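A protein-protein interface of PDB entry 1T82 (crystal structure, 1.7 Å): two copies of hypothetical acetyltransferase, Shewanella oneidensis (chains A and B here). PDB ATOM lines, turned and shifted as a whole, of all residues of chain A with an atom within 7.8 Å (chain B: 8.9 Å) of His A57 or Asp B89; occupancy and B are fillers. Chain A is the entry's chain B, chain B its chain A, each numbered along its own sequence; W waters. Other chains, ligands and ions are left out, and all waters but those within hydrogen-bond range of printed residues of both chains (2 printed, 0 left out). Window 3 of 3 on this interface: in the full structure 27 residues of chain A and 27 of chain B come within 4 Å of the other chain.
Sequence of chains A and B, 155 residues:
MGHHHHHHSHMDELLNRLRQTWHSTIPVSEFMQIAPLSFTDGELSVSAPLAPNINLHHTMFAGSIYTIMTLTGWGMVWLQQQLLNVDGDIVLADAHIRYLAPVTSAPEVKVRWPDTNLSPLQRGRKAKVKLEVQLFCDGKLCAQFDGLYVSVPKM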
ATOM      1  N   LEU A  50     -11.602 -43.673  36.371  1.00  0.00           N
ATOM      2  CA  LEU A  50     -11.093 -42.621  35.519  1.00  0.00           C
ATOM      3  C   LEU A  50     -10.285 -43.178  34.348  1.00  0.00           C
ATOM      4  O   LEU A  50     -10.414 -42.705  33.225  1.00  0.00           O
ATOM      5  CB  LEU A  50     -10.225 -41.667  36.339  1.00  0.00           C
ATOM      6  CG  LEU A  50      -9.634 -40.468  35.602  1.00  0.00           C
ATOM      7  CD1 LEU A  50     -10.739 -39.673  34.901  1.00  0.00           C
ATOM      8  CD2 LEU A  50      -8.895 -39.593  36.607  1.00  0.00           C
ATOM      9  N   ILE A  54     -10.166 -41.192  30.500  1.00  0.00           N
ATOM     10  CA  ILE A  54      -9.328 -39.999  30.529  1.00  0.00           C
ATOM     11  C   ILE A  54      -9.233 -39.216  29.218  1.00  0.00           C
ATOM     12  O   ILE A  54      -9.676 -39.666  28.153  1.00  0.00           O
ATOM     13  CB  ILE A  54      -7.885 -40.338  30.982  1.00  0.00           C
ATOM     14  CG1 ILE A  54      -7.242 -41.336  30.011  1.00  0.00           C
ATOM     15  CG2 ILE A  54      -7.911 -40.928  32.385  1.00  0.00           C
ATOM     16  CD1 ILE A  54      -5.793 -41.682  30.356  1.00  0.00           C
ATOM     17  N   ASN A  55      -8.667 -38.020  29.337  1.00  0.00           N
ATOM     18  CA  ASN A  55      -8.417 -37.126  28.216  1.00  0.00           C
ATOM     19  C   ASN A  55      -6.932 -36.789  28.348  1.00  0.00           C
ATOM     20  O   ASN A  55      -6.242 -37.372  29.184  1.00  0.00           O
ATOM     21  CB  ASN A  55      -9.264 -35.854  28.319  1.00  0.00           C
ATOM     22  CG  ASN A  55      -9.082 -35.141  29.641  1.00  0.00           C
ATOM     23  OD1 ASN A  55      -8.014 -35.198  30.245  1.00  0.00           O
ATOM     24  ND2 ASN A  55     -10.131 -34.452  30.095  1.00  0.00           N
ATOM     25  N   LEU A  56      -6.442 -35.849  27.549  1.00  0.00           N
ATOM     26  CA  LEU A  56      -5.029 -35.481  27.589  1.00  0.00           C
ATOM     27  C   LEU A  56      -4.554 -34.932  28.934  1.00  0.00           C
ATOM     28  O   LEU A  56      -3.364 -35.002  29.252  1.00  0.00           O
ATOM     29  CB  LEU A  56      -4.719 -34.476  26.471  1.00  0.00           C
ATOM     30  CG  LEU A  56      -5.291 -33.056  26.517  1.00  0.00           C
ATOM     31  CD1 LEU A  56      -4.359 -32.150  27.314  1.00  0.00           C
ATOM     32  CD2 LEU A  56      -5.428 -32.522  25.098  1.00  0.00           C
ATOM     33  N   HIS A  57      -5.475 -34.385  29.718  1.00  0.00           N
ATOM     34  CA  HIS A  57      -5.135 -33.828  31.028  1.00  0.00           C
ATOM     35  C   HIS A  57      -5.168 -34.904  32.104  1.00  0.00           C
ATOM     36  O   HIS A  57      -4.869 -34.637  33.270  1.00  0.00           O
ATOM     37  CB  HIS A  57      -6.129 -32.731  31.427  1.00  0.00           C
ATOM     38  CG  HIS A  57      -6.275 -31.640  30.414  1.00  0.00           C
ATOM     39  ND1 HIS A  57      -7.299 -31.612  29.493  1.00  0.00           N
ATOM     40  CD2 HIS A  57      -5.530 -30.535  30.183  1.00  0.00           C
ATOM     41  CE1 HIS A  57      -7.180 -30.535  28.738  1.00  0.00           C
ATOM     42  NE2 HIS A  57      -6.114 -29.864  29.137  1.00  0.00           N
ATOM     43  N   HIS A  58      -5.531 -36.118  31.710  1.00  0.00           N
ATOM     44  CA  HIS A  58      -5.638 -37.217  32.654  1.00  0.00           C
ATOM     45  C   HIS A  58      -6.813 -36.970  33.604  1.00  0.00           C
ATOM     46  O   HIS A  58      -6.849 -37.499  34.716  1.00  0.00           O
ATOM     47  CB  HIS A  58      -4.329 -37.397  33.436  1.00  0.00           C
ATOM     48  CG  HIS A  58      -3.253 -38.076  32.648  1.00  0.00           C
ATOM     49  ND1 HIS A  58      -3.160 -39.447  32.543  1.00  0.00           N
ATOM     50  CD2 HIS A  58      -2.259 -37.572  31.880  1.00  0.00           C
ATOM     51  CE1 HIS A  58      -2.156 -39.759  31.744  1.00  0.00           C
ATOM     52  NE2 HIS A  58      -1.593 -38.639  31.327  1.00  0.00           N
ATOM     53  N   THR A  59      -7.758 -36.139  33.166  1.00  0.00           N
ATOM     54  CA  THR A  59      -8.971 -35.869  33.942  1.00  0.00           C
ATOM     55  C   THR A  59     -10.080 -36.537  33.145  1.00  0.00           C
ATOM     56  O   THR A  59      -9.824 -37.024  32.046  1.00  0.00           O
ATOM     57  CB  THR A  59      -9.266 -34.357  34.100  1.00  0.00           C
ATOM     58  OG1 THR A  59      -9.322 -33.725  32.816  1.00  0.00           O
ATOM     59  CG2 THR A  59      -8.191 -33.703  34.955  1.00  0.00           C
ATOM     60  N   MET A  60     -11.306 -36.573  33.653  1.00  0.00           N
ATOM     61  CA  MET A  60     -12.329 -37.273  32.883  1.00  0.00           C
ATOM     62  C   MET A  60     -12.780 -36.567  31.608  1.00  0.00           C
ATOM     63  O   MET A  60     -13.095 -35.375  31.598  1.00  0.00           O
ATOM     64  CB  MET A  60     -13.542 -37.617  33.751  1.00  0.00           C
ATOM     65  CG  MET A  60     -14.403 -38.721  33.121  1.00  0.00           C
ATOM     66  SD  MET A  60     -15.854 -39.364  34.233  1.00  0.00           S
ATOM     67  CE  MET A  60     -14.870 -40.821  35.056  1.00  0.00           C
ATOM     68  N   PRO A 102     -12.866 -29.830  36.449  1.00  0.00           N
ATOM     69  CA  PRO A 102     -12.302 -31.111  36.020  1.00  0.00           C
ATOM     70  C   PRO A 102     -12.560 -32.220  37.040  1.00  0.00           C
ATOM     71  O   PRO A 102     -12.615 -31.969  38.250  1.00  0.00           O
ATOM     72  CB  PRO A 102     -10.809 -30.800  35.875  1.00  0.00           C
ATOM     73  CG  PRO A 102     -10.802 -29.346  35.501  1.00  0.00           C
ATOM     74  CD  PRO A 102     -11.835 -28.777  36.451  1.00  0.00           C
ATOM     75  N   VAL A 103     -12.732 -33.439  36.537  1.00  0.00           N
ATOM     76  CA  VAL A 103     -12.971 -34.615  37.364  1.00  0.00           C
ATOM     77  C   VAL A 103     -11.642 -35.350  37.475  1.00  0.00           C
ATOM     78  O   VAL A 103     -11.132 -35.879  36.488  1.00  0.00           O
ATOM     79  CB  VAL A 103     -14.017 -35.549  36.718  1.00  0.00           C
ATOM     80  CG1 VAL A 103     -14.206 -36.791  37.568  1.00  0.00           C
ATOM     81  CG2 VAL A 103     -15.336 -34.812  36.546  1.00  0.00           C
ATOM     82  N   THR A 104     -11.093 -35.395  38.685  1.00  0.00           N
ATOM     83  CA  THR A 104      -9.792 -36.014  38.918  1.00  0.00           C
ATOM     84  C   THR A 104      -9.739 -37.435  39.474  1.00  0.00           C
ATOM     85  O   THR A 104      -8.655 -37.971  39.716  1.00  0.00           O
ATOM     86  CB  THR A 104      -8.943 -35.105  39.813  1.00  0.00           C
ATOM     87  OG1 THR A 104      -9.666 -34.812  41.015  1.00  0.00           O
ATOM     88  CG2 THR A 104      -8.627 -33.811  39.087  1.00  0.00           C
ATOM     89  N   THR B  25      -4.922 -39.749  23.068  1.00  0.00           N
ATOM     90  CA  THR B  25      -5.218 -39.056  24.321  1.00  0.00           C
ATOM     91  C   THR B  25      -6.568 -39.378  24.952  1.00  0.00           C
ATOM     92  O   THR B  25      -6.777 -39.127  26.143  1.00  0.00           O
ATOM     93  CB  THR B  25      -5.144 -37.519  24.141  1.00  0.00           C
ATOM     94  OG1 THR B  25      -6.165 -37.092  23.229  1.00  0.00           O
ATOM     95  CG2 THR B  25      -3.783 -37.112  23.604  1.00  0.00           C
ATOM     96  N   ILE B  26      -7.479 -39.930  24.158  1.00  0.00           N
ATOM     97  CA  ILE B  26      -8.817 -40.261  24.644  1.00  0.00           C
ATOM     98  C   ILE B  26      -9.168 -41.703  24.299  1.00  0.00           C
ATOM     99  O   ILE B  26      -9.718 -41.975  23.228  1.00  0.00           O
ATOM    100  CB  ILE B  26      -9.866 -39.333  23.997  1.00  0.00           C
ATOM    101  CG1 ILE B  26      -9.437 -37.873  24.180  1.00  0.00           C
ATOM    102  CG2 ILE B  26     -11.233 -39.585  24.613  1.00  0.00           C
ATOM    103  CD1 ILE B  26     -10.280 -36.886  23.410  1.00  0.00           C
ATOM    104  N   TRP B  74     -14.784 -30.217  18.737  1.00  0.00           N
ATOM    105  CA  TRP B  74     -13.412 -30.131  19.233  1.00  0.00           C
ATOM    106  C   TRP B  74     -12.458 -30.081  18.037  1.00  0.00           C
ATOM    107  O   TRP B  74     -11.548 -29.252  17.981  1.00  0.00           O
ATOM    108  CB  TRP B  74     -13.098 -31.369  20.089  1.00  0.00           C
ATOM    109  CG  TRP B  74     -11.840 -31.295  20.929  1.00  0.00           C
ATOM    110  CD1 TRP B  74     -11.764 -31.030  22.270  1.00  0.00           C
ATOM    111  CD2 TRP B  74     -10.497 -31.543  20.496  1.00  0.00           C
ATOM    112  NE1 TRP B  74     -10.459 -31.106  22.698  1.00  0.00           N
ATOM    113  CE2 TRP B  74      -9.661 -31.418  21.630  1.00  0.00           C
ATOM    114  CE3 TRP B  74      -9.917 -31.859  19.262  1.00  0.00           C
ATOM    115  CZ2 TRP B  74      -8.273 -31.600  21.565  1.00  0.00           C
ATOM    116  CZ3 TRP B  74      -8.535 -32.041  19.198  1.00  0.00           C
ATOM    117  CH2 TRP B  74      -7.732 -31.911  20.345  1.00  0.00           C
ATOM    118  N   VAL B  77     -12.369 -26.721  16.211  1.00  0.00           N
ATOM    119  CA  VAL B  77     -11.594 -25.713  16.930  1.00  0.00           C
ATOM    120  C   VAL B  77     -10.108 -25.980  16.689  1.00  0.00           C
ATOM    121  O   VAL B  77      -9.340 -25.063  16.414  1.00  0.00           O
ATOM    122  CB  VAL B  77     -11.873 -25.752  18.453  1.00  0.00           C
ATOM    123  CG1 VAL B  77     -11.027 -24.699  19.164  1.00  0.00           C
ATOM    124  CG2 VAL B  77     -13.352 -25.501  18.719  1.00  0.00           C
ATOM    125  N   TRP B  78      -9.717 -27.247  16.780  1.00  0.00           N
ATOM    126  CA  TRP B  78      -8.331 -27.647  16.573  1.00  0.00           C
ATOM    127  C   TRP B  78      -7.868 -27.227  15.179  1.00  0.00           C
ATOM    128  O   TRP B  78      -6.778 -26.669  15.013  1.00  0.00           O
ATOM    129  CB  TRP B  78      -8.215 -29.163  16.725  1.00  0.00           C
ATOM    130  CG  TRP B  78      -6.819 -29.716  16.699  1.00  0.00           C
ATOM    131  CD1 TRP B  78      -5.953 -29.825  17.753  1.00  0.00           C
ATOM    132  CD2 TRP B  78      -6.169 -30.329  15.581  1.00  0.00           C
ATOM    133  NE1 TRP B  78      -4.805 -30.483  17.360  1.00  0.00           N
ATOM    134  CE2 TRP B  78      -4.914 -30.801  16.032  1.00  0.00           C
ATOM    135  CE3 TRP B  78      -6.527 -30.528  14.241  1.00  0.00           C
ATOM    136  CZ2 TRP B  78      -4.017 -31.463  15.188  1.00  0.00           C
ATOM    137  CZ3 TRP B  78      -5.636 -31.186  13.400  1.00  0.00           C
ATOM    138  CH2 TRP B  78      -4.395 -31.646  13.880  1.00  0.00           C
ATOM    139  N   GLN B  81      -7.427 -23.568  14.896  1.00  0.00           N
ATOM    140  CA  GLN B  81      -6.215 -23.145  15.586  1.00  0.00           C
ATOM    141  C   GLN B  81      -5.032 -23.353  14.639  1.00  0.00           C
ATOM    142  O   GLN B  81      -4.144 -22.506  14.544  1.00  0.00           O
ATOM    143  CB  GLN B  81      -6.003 -23.953  16.870  1.00  0.00           C
ATOM    144  CG  GLN B  81      -6.926 -23.564  18.014  1.00  0.00           C
ATOM    145  CD  GLN B  81      -6.557 -24.257  19.311  1.00  0.00           C
ATOM    146  OE1 GLN B  81      -5.487 -24.852  19.425  1.00  0.00           O
ATOM    147  NE2 GLN B  81      -7.434 -24.168  20.304  1.00  0.00           N
ATOM    148  N   VAL B  86      -1.962 -20.998  15.929  1.00  0.00           N
ATOM    149  CA  VAL B  86      -1.971 -20.758  17.362  1.00  0.00           C
ATOM    150  C   VAL B  86      -2.323 -22.064  18.054  1.00  0.00           C
ATOM    151  O   VAL B  86      -2.754 -23.018  17.405  1.00  0.00           O
ATOM    152  CB  VAL B  86      -3.012 -19.684  17.748  1.00  0.00           C
ATOM    153  CG1 VAL B  86      -2.650 -18.356  17.101  1.00  0.00           C
ATOM    154  CG2 VAL B  86      -4.404 -20.125  17.311  1.00  0.00           C
ATOM    155  N   ASP B  87      -2.120 -22.112  19.367  1.00  0.00           N
ATOM    156  CA  ASP B  87      -2.437 -23.305  20.144  1.00  0.00           C
ATOM    157  C   ASP B  87      -3.128 -22.914  21.439  1.00  0.00           C
ATOM    158  O   ASP B  87      -2.917 -21.823  21.967  1.00  0.00           O
ATOM    159  CB  ASP B  87      -1.175 -24.106  20.473  1.00  0.00           C
ATOM    160  CG  ASP B  87      -1.451 -25.263  21.421  1.00  0.00           C
ATOM    161  OD1 ASP B  87      -2.242 -26.162  21.057  1.00  0.00           O
ATOM    162  OD2 ASP B  87      -0.886 -25.276  22.537  1.00  0.00           O
ATOM    163  N   GLY B  88      -3.960 -23.816  21.947  1.00  0.00           N
ATOM    164  CA  GLY B  88      -4.666 -23.552  23.184  1.00  0.00           C
ATOM    165  C   GLY B  88      -5.471 -24.753  23.632  1.00  0.00           C
ATOM    166  O   GLY B  88      -5.915 -25.555  22.813  1.00  0.00           O
ATOM    167  N   ASP B  89      -5.647 -24.885  24.942  1.00  0.00           N
ATOM    168  CA  ASP B  89      -6.422 -25.983  25.498  1.00  0.00           C
ATOM    169  C   ASP B  89      -7.867 -25.810  25.037  1.00  0.00           C
ATOM    170  O   ASP B  89      -8.445 -24.734  25.179  1.00  0.00           O
ATOM    171  CB  ASP B  89      -6.330 -25.952  27.028  1.00  0.00           C
ATOM    172  CG  ASP B  89      -7.096 -27.079  27.685  1.00  0.00           C
ATOM    173  OD1 ASP B  89      -7.160 -28.176  27.097  1.00  0.00           O
ATOM    174  OD2 ASP B  89      -7.619 -26.869  28.800  1.00  0.00           O
ATOM    175  N   ILE B  90      -8.440 -26.868  24.471  1.00  0.00           N
ATOM    176  CA  ILE B  90      -9.815 -26.832  23.976  1.00  0.00           C
ATOM    177  C   ILE B  90     -10.751 -27.432  25.016  1.00  0.00           C
ATOM    178  O   ILE B  90     -10.682 -28.628  25.302  1.00  0.00           O
ATOM    179  CB  ILE B  90      -9.947 -27.636  22.668  1.00  0.00           C
ATOM    180  CG1 ILE B  90      -8.953 -27.090  21.634  1.00  0.00           C
ATOM    181  CG2 ILE B  90     -11.379 -27.554  22.143  1.00  0.00           C
ATOM    182  CD1 ILE B  90      -8.848 -27.924  20.374  1.00  0.00           C
ATOM    183  N   VAL B  91     -11.635 -26.608  25.572  1.00  0.00           N
ATOM    184  CA  VAL B  91     -12.553 -27.086  26.597  1.00  0.00           C
ATOM    185  C   VAL B  91     -14.027 -26.851  26.267  1.00  0.00           C
ATOM    186  O   VAL B  91     -14.414 -25.765  25.831  1.00  0.00           O
ATOM    187  CB  VAL B  91     -12.230 -26.418  27.960  1.00  0.00           C
ATOM    188  CG1 VAL B  91     -13.096 -27.014  29.055  1.00  0.00           C
ATOM    189  CG2 VAL B  91     -10.754 -26.601  28.291  1.00  0.00           C
ATOM    190  N   LEU B  92     -14.848 -27.882  26.459  1.00  0.00           N
ATOM    191  CA  LEU B  92     -16.287 -27.771  26.214  1.00  0.00           C
ATOM    192  C   LEU B  92     -16.915 -27.290  27.524  1.00  0.00           C
ATOM    193  O   LEU B  92     -16.900 -28.009  28.524  1.00  0.00           O
ATOM    194  CB  LEU B  92     -16.870 -29.135  25.816  1.00  0.00           C
ATOM    195  CG  LEU B  92     -18.384 -29.194  25.563  1.00  0.00           C
ATOM    196  CD1 LEU B  92     -18.773 -28.221  24.452  1.00  0.00           C
ATOM    197  CD2 LEU B  92     -18.776 -30.614  25.180  1.00  0.00           C
ATOM    198  N   LEU B 121      -6.561 -15.584  20.770  1.00  0.00           N
ATOM    199  CA  LEU B 121      -5.462 -16.493  21.065  1.00  0.00           C
ATOM    200  C   LEU B 121      -4.134 -15.896  20.612  1.00  0.00           C
ATOM    201  O   LEU B 121      -3.088 -16.177  21.196  1.00  0.00           O
ATOM    202  CB  LEU B 121      -5.686 -17.838  20.368  1.00  0.00           C
ATOM    203  CG  LEU B 121      -6.857 -18.683  20.874  1.00  0.00           C
ATOM    204  CD1 LEU B 121      -7.052 -19.897  19.973  1.00  0.00           C
ATOM    205  CD2 LEU B 121      -6.586 -19.115  22.305  1.00  0.00           C
ATOM    206  N   LYS B 126      -8.092 -15.947  25.880  1.00  0.00           N
ATOM    207  CA  LYS B 126      -8.963 -17.070  25.558  1.00  0.00           C
ATOM    208  C   LYS B 126      -9.972 -16.686  24.482  1.00  0.00           C
ATOM    209  O   LYS B 126     -10.419 -15.541  24.408  1.00  0.00           O
ATOM    210  CB  LYS B 126      -9.687 -17.566  26.812  1.00  0.00           C
ATOM    211  CG  LYS B 126     -10.714 -16.619  27.392  1.00  0.00           C
ATOM    212  CD  LYS B 126     -11.381 -17.259  28.598  1.00  0.00           C
ATOM    213  CE  LYS B 126     -12.547 -16.433  29.108  1.00  0.00           C
ATOM    214  NZ  LYS B 126     -13.261 -17.156  30.197  1.00  0.00           N
ATOM    215  N   ALA B 127     -10.321 -17.648  23.636  1.00  0.00           N
ATOM    216  CA  ALA B 127     -11.276 -17.399  22.564  1.00  0.00           C
ATOM    217  C   ALA B 127     -12.427 -18.388  22.661  1.00  0.00           C
ATOM    218  O   ALA B 127     -12.214 -19.597  22.691  1.00  0.00           O
ATOM    219  CB  ALA B 127     -10.588 -17.526  21.214  1.00  0.00           C
ATOM    220  N   TYR B 149     -17.384 -23.941  23.058  1.00  0.00           N
ATOM    221  CA  TYR B 149     -15.987 -24.334  23.187  1.00  0.00           C
ATOM    222  C   TYR B 149     -15.120 -23.131  23.476  1.00  0.00           C
ATOM    223  O   TYR B 149     -15.285 -22.077  22.870  1.00  0.00           O
ATOM    224  CB  TYR B 149     -15.476 -24.984  21.906  1.00  0.00           C
ATOM    225  CG  TYR B 149     -16.123 -26.302  21.585  1.00  0.00           C
ATOM    226  CD1 TYR B 149     -17.366 -26.354  20.958  1.00  0.00           C
ATOM    227  CD2 TYR B 149     -15.483 -27.504  21.900  1.00  0.00           C
ATOM    228  CE1 TYR B 149     -17.957 -27.569  20.643  1.00  0.00           C
ATOM    229  CE2 TYR B 149     -16.067 -28.727  21.595  1.00  0.00           C
ATOM    230  CZ  TYR B 149     -17.305 -28.748  20.963  1.00  0.00           C
ATOM    231  OH  TYR B 149     -17.892 -29.943  20.638  1.00  0.00           O
ATOM    232  N   VAL B 150     -14.180 -23.301  24.391  1.00  0.00           N
ATOM    233  CA  VAL B 150     -13.281 -22.220  24.744  1.00  0.00           C
ATOM    234  C   VAL B 150     -11.842 -22.653  24.508  1.00  0.00           C
ATOM    235  O   VAL B 150     -11.451 -23.762  24.874  1.00  0.00           O
ATOM    236  CB  VAL B 150     -13.453 -21.827  26.225  1.00  0.00           C
ATOM    237  CG1 VAL B 150     -12.567 -20.639  26.555  1.00  0.00           C
ATOM    238  CG2 VAL B 150     -14.918 -21.499  26.505  1.00  0.00           C
ATOM    239  N   SER B 151     -11.058 -21.784  23.878  1.00  0.00           N
ATOM    240  CA  SER B 151      -9.651 -22.078  23.635  1.00  0.00           C
ATOM    241  C   SER B 151      -8.860 -21.224  24.615  1.00  0.00           C
ATOM    242  O   SER B 151      -8.958 -19.999  24.596  1.00  0.00           O
ATOM    243  CB  SER B 151      -9.258 -21.732  22.193  1.00  0.00           C
ATOM    244  OG  SER B 151      -9.806 -22.667  21.273  1.00  0.00           O
ATOM    245  N   VAL B 152      -8.094 -21.880  25.480  1.00  0.00           N
ATOM    246  CA  VAL B 152      -7.297 -21.186  26.486  1.00  0.00           C
ATOM    247  C   VAL B 152      -5.807 -21.314  26.176  1.00  0.00           C
ATOM    248  O   VAL B 152      -5.236 -22.402  26.255  1.00  0.00           O
ATOM    249  CB  VAL B 152      -7.563 -21.763  27.896  1.00  0.00           C
ATOM    250  CG1 VAL B 152      -6.864 -20.918  28.949  1.00  0.00           C
ATOM    251  CG2 VAL B 152      -9.058 -21.820  28.162  1.00  0.00           C
ATOM    252  N   PRO B 153      -5.160 -20.193  25.815  1.00  0.00           N
ATOM    253  CA  PRO B 153      -3.732 -20.147  25.484  1.00  0.00           C
ATOM    254  C   PRO B 153      -2.834 -20.429  26.687  1.00  0.00           C
ATOM    255  O   PRO B 153      -1.735 -20.992  26.482  1.00  0.00           O
ATOM    256  CB  PRO B 153      -3.556 -18.736  24.935  1.00  0.00           C
ATOM    257  CG  PRO B 153      -4.545 -17.953  25.730  1.00  0.00           C
ATOM    258  CD  PRO B 153      -5.762 -18.852  25.713  1.00  0.00           C
HETATM  259  O   HOH W   1      -4.436 -39.361  27.861  1.00  0.00           O
HETATM  260  O   HOH W   2      -7.610 -35.268  25.018  1.00  0.00           O
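No position is printed for both chains.
Leu A56 touches just one residue of chain B: Thr B25 (3.6 Å). His A57 touches just one residue of chain B: Asp B89. Of the printed residues of chain A, Thr B25 touches Ile A54 (3.6 Å), Asn A55 (3.2 Å) and Leu A56 (3.6 Å). Of the printed residues of chain A, Ile B26 touches Ile A54. No residue of chain A comes within 4 Å of Gly B88. The nearest printed residue of chain B that does not touch Asn A55 is Ile B26 (4.2 Å).
Water W2 lies within hydrogen-bond range of N of Leu A56 (2.8 Å) and OG1 of Thr B25 (2.9 Å). Water W1 bridges the backbone carbonyl oxygen of Thr B25 (2.9 Å) and the backbone carbonyl oxygen of Asn A55 (3.0 Å).
The backbone NH of Asp B89 sits at hydrogen-bond distance from the backbone carbonyl oxygen of Val B152. The backbone NH of His A57 sits at hydrogen-bond distance from the side-chain amide oxygen of Asn A55, 2.7 Å away. OD1 of Asn A55 lies within hydrogen-bond range of N of His A58 (3.0 Å). The side-chain hydroxyl (OG1) of Thr A59 is in hydrogen-bond range of the side-chain amide nitrogen (ND2) of Asn A55 (2.9 Å). The side-chain amide nitrogen (ND2) of Asn A55 is in hydrogen-bond range of the backbone carbonyl oxygen (O) of Met A60 (3.4 Å).
Of the 21 printed residues of chain B, 3 touch a printed residue of chain A. Hydrophobic or aromatic side chains of chain B that line the printed part of chain A: Ile B26. Hydrophobic or aromatic side chains of chain A that line the printed part of chain B: Leu A56 and His A57.
The side-chain carboxylate of Asp B89 is in hydrogen-bond range of a ring nitrogen (NE2) of His A57 (2.8 Å).
Thr B25 touches Ile A54. O of Ile A54 touches CA of Ile B26, at 3.7 Å. C of Asn A55 touches O of Thr B25, 3.2 Å away. Thr B25 touches Leu A56.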
